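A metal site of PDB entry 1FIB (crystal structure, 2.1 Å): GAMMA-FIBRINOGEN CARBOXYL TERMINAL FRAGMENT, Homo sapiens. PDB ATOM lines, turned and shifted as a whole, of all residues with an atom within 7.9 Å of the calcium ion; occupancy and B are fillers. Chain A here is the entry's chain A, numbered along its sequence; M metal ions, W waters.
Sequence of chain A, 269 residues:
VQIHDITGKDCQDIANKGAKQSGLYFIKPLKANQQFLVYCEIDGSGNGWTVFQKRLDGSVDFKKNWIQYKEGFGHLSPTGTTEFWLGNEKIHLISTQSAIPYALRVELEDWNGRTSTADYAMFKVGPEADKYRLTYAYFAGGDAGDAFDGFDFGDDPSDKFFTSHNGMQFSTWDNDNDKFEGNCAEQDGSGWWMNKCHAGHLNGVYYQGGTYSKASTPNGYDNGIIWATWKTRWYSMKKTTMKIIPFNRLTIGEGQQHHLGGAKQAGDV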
ATOM      1  N   SER A 171       9.821  17.405  26.110  1.00  0.00           N
ATOM      2  CA  SER A 171       8.748  17.605  25.127  1.00  0.00           C
ATOM      3  C   SER A 171       7.488  18.276  25.704  1.00  0.00           C
ATOM      4  O   SER A 171       7.101  18.008  26.839  1.00  0.00           O
ATOM      5  CB  SER A 171       8.289  16.265  24.517  1.00  0.00           C
ATOM      6  OG  SER A 171       9.214  15.746  23.590  1.00  0.00           O
ATOM      7  N   ASN A 175       6.350  21.041  20.738  1.00  0.00           N
ATOM      8  CA  ASN A 175       7.782  20.820  20.551  1.00  0.00           C
ATOM      9  C   ASN A 175       8.011  19.372  20.934  1.00  0.00           C
ATOM     10  O   ASN A 175       8.369  19.047  22.060  1.00  0.00           O
ATOM     11  CB  ASN A 175       8.601  21.749  21.453  1.00  0.00           C
ATOM     12  CG  ASN A 175       9.999  21.997  20.907  1.00  0.00           C
ATOM     13  OD1 ASN A 175      10.786  21.079  20.738  1.00  0.00           O
ATOM     14  ND2 ASN A 175      10.302  23.258  20.640  1.00  0.00           N
ATOM     15  N   ASP A 176       7.756  18.504  19.957  1.00  0.00           N
ATOM     16  CA  ASP A 176       7.871  17.064  20.089  1.00  0.00           C
ATOM     17  C   ASP A 176       9.314  16.603  19.893  1.00  0.00           C
ATOM     18  O   ASP A 176       9.891  16.795  18.829  1.00  0.00           O
ATOM     19  CB  ASP A 176       6.946  16.404  19.060  1.00  0.00           C
ATOM     20  CG  ASP A 176       6.906  14.904  19.167  1.00  0.00           C
ATOM     21  OD1 ASP A 176       7.728  14.320  19.888  1.00  0.00           O
ATOM     22  OD2 ASP A 176       6.040  14.282  18.533  1.00  0.00           O
ATOM     23  N   ASN A 177       9.877  15.964  20.923  1.00  0.00           N
ATOM     24  CA  ASN A 177      11.249  15.485  20.885  1.00  0.00           C
ATOM     25  C   ASN A 177      11.319  14.100  21.503  1.00  0.00           C
ATOM     26  O   ASN A 177      12.360  13.692  22.010  1.00  0.00           O
ATOM     27  CB  ASN A 177      12.180  16.417  21.677  1.00  0.00           C
ATOM     28  CG  ASN A 177      12.189  17.842  21.141  1.00  0.00           C
ATOM     29  OD1 ASN A 177      12.641  18.080  20.015  1.00  0.00           O
ATOM     30  ND2 ASN A 177      11.713  18.799  21.944  1.00  0.00           N
ATOM     31  N   ASP A 178      10.193  13.391  21.529  1.00  0.00           N
ATOM     32  CA  ASP A 178      10.145  12.063  22.117  1.00  0.00           C
ATOM     33  C   ASP A 178      10.567  10.988  21.100  1.00  0.00           C
ATOM     34  O   ASP A 178      10.950  11.292  19.975  1.00  0.00           O
ATOM     35  CB  ASP A 178       8.753  11.767  22.689  1.00  0.00           C
ATOM     36  CG  ASP A 178       7.635  11.765  21.640  1.00  0.00           C
ATOM     37  OD1 ASP A 178       7.881  11.414  20.461  1.00  0.00           O
ATOM     38  OD2 ASP A 178       6.488  12.121  21.982  1.00  0.00           O
ATOM     39  N   LYS A 179      10.461   9.730  21.503  1.00  0.00           N
ATOM     40  CA  LYS A 179      10.828   8.613  20.639  1.00  0.00           C
ATOM     41  C   LYS A 179       9.590   7.907  20.069  1.00  0.00           C
ATOM     42  O   LYS A 179       9.670   6.766  19.606  1.00  0.00           O
ATOM     43  CB  LYS A 179      11.658   7.618  21.452  1.00  0.00           C
ATOM     44  CG  LYS A 179      12.939   8.230  22.008  1.00  0.00           C
ATOM     45  CD  LYS A 179      14.125   7.753  21.195  1.00  0.00           C
ATOM     46  CE  LYS A 179      15.432   8.357  21.705  1.00  0.00           C
ATOM     47  NZ  LYS A 179      15.500   9.826  21.441  1.00  0.00           N
ATOM     48  N   PHE A 180       8.452   8.587  20.092  1.00  0.00           N
ATOM     49  CA  PHE A 180       7.176   8.058  19.623  1.00  0.00           C
ATOM     50  C   PHE A 180       6.785   8.608  18.234  1.00  0.00           C
ATOM     51  O   PHE A 180       7.116   9.743  17.877  1.00  0.00           O
ATOM     52  CB  PHE A 180       6.099   8.431  20.648  1.00  0.00           C
ATOM     53  CG  PHE A 180       4.729   7.856  20.375  1.00  0.00           C
ATOM     54  CD1 PHE A 180       4.580   6.592  19.811  1.00  0.00           C
ATOM     55  CD2 PHE A 180       3.584   8.583  20.696  1.00  0.00           C
ATOM     56  CE1 PHE A 180       3.308   6.066  19.573  1.00  0.00           C
ATOM     57  CE2 PHE A 180       2.303   8.065  20.464  1.00  0.00           C
ATOM     58  CZ  PHE A 180       2.164   6.799  19.902  1.00  0.00           C
ATOM     59  N   GLU A 181       6.083   7.786  17.463  1.00  0.00           N
ATOM     60  CA  GLU A 181       5.612   8.157  16.133  1.00  0.00           C
ATOM     61  C   GLU A 181       4.553   9.248  16.295  1.00  0.00           C
ATOM     62  O   GLU A 181       4.364  10.091  15.412  1.00  0.00           O
ATOM     63  CB  GLU A 181       4.994   6.950  15.404  1.00  0.00           C
ATOM     64  CG  GLU A 181       5.961   5.801  15.148  1.00  0.00           C
ATOM     65  CD  GLU A 181       5.782   4.630  16.128  1.00  0.00           C
ATOM     66  OE1 GLU A 181       6.221   4.742  17.295  1.00  0.00           O
ATOM     67  OE2 GLU A 181       5.205   3.597  15.708  1.00  0.00           O
ATOM     68  N   GLY A 182       3.817   9.164  17.404  1.00  0.00           N
ATOM     69  CA  GLY A 182       2.809  10.176  17.721  1.00  0.00           C
ATOM     70  C   GLY A 182       3.419  11.266  18.598  1.00  0.00           C
ATOM     71  O   GLY A 182       4.649  11.429  18.656  1.00  0.00           O
ATOM     72  N   ASN A 183       2.577  11.978  19.338  1.00  0.00           N
ATOM     73  CA  ASN A 183       3.041  13.050  20.195  1.00  0.00           C
ATOM     74  C   ASN A 183       2.619  12.741  21.623  1.00  0.00           C
ATOM     75  O   ASN A 183       1.449  12.918  21.984  1.00  0.00           O
ATOM     76  CB  ASN A 183       2.454  14.400  19.720  1.00  0.00           C
ATOM     77  CG  ASN A 183       3.040  15.612  20.458  1.00  0.00           C
ATOM     78  OD1 ASN A 183       3.522  15.510  21.580  1.00  0.00           O
ATOM     79  ND2 ASN A 183       2.976  16.767  19.808  1.00  0.00           N
ATOM     80  N   CYS A 184       3.547  12.228  22.426  1.00  0.00           N
ATOM     81  CA  CYS A 184       3.277  11.885  23.828  1.00  0.00           C
ATOM     82  C   CYS A 184       2.740  13.086  24.639  1.00  0.00           C
ATOM     83  O   CYS A 184       1.748  12.967  25.354  1.00  0.00           O
ATOM     84  CB  CYS A 184       4.545  11.366  24.510  1.00  0.00           C
ATOM     85  SG  CYS A 184       5.137   9.724  24.035  1.00  0.00           S
ATOM     86  N   ALA A 185       3.432  14.218  24.547  1.00  0.00           N
ATOM     87  CA  ALA A 185       3.045  15.402  25.304  1.00  0.00           C
ATOM     88  C   ALA A 185       1.647  15.915  24.966  1.00  0.00           C
ATOM     89  O   ALA A 185       0.930  16.398  25.841  1.00  0.00           O
ATOM     90  CB  ALA A 185       4.058  16.497  25.094  1.00  0.00           C
ATOM     91  N   ASN A 195       9.595   9.398  26.365  1.00  0.00           N
ATOM     92  CA  ASN A 195      10.273   8.376  25.571  1.00  0.00           C
ATOM     93  C   ASN A 195       9.205   7.888  24.573  1.00  0.00           C
ATOM     94  O   ASN A 195       8.791   8.653  23.694  1.00  0.00           O
ATOM     95  CB  ASN A 195      10.742   7.226  26.481  1.00  0.00           C
ATOM     96  CG  ASN A 195      11.625   6.236  25.747  1.00  0.00           C
ATOM     97  OD1 ASN A 195      11.542   6.095  24.519  1.00  0.00           O
ATOM     98  ND2 ASN A 195      12.483   5.542  26.480  1.00  0.00           N
HETATM   99 CA    CA M   1       7.028  12.061  18.343  1.00  0.00          CA
HETATM  100  O   HOH W   1       9.490  12.465  17.904  1.00  0.00           O
HETATM  101  O   HOH W   2       6.765  12.478  15.908  1.00  0.00           O
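N of Asp 178 lies within hydrogen-bond range of OG of Ser 171 (3.3 Å).
OD2 of Asp 178 is in hydrogen-bond range of N of Cys 184, 3.0 Å away.
The nearest printed residue that does not touch the calcium ion is Glu 181 (4.3 Å).
The calcium ion is bound by O of Phe 180 (2.4 Å), OD1 of Asp 178 (2.4 Å), OD2 of Asp 176 (2.4 Å), O of Gly 182 (2.5 Å), water W2 (2.5 Å), water W1 (2.5 Å) and OD1 of Asp 176 (2.8 Å).
The calcium ion has seven donor atoms within binding distance.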
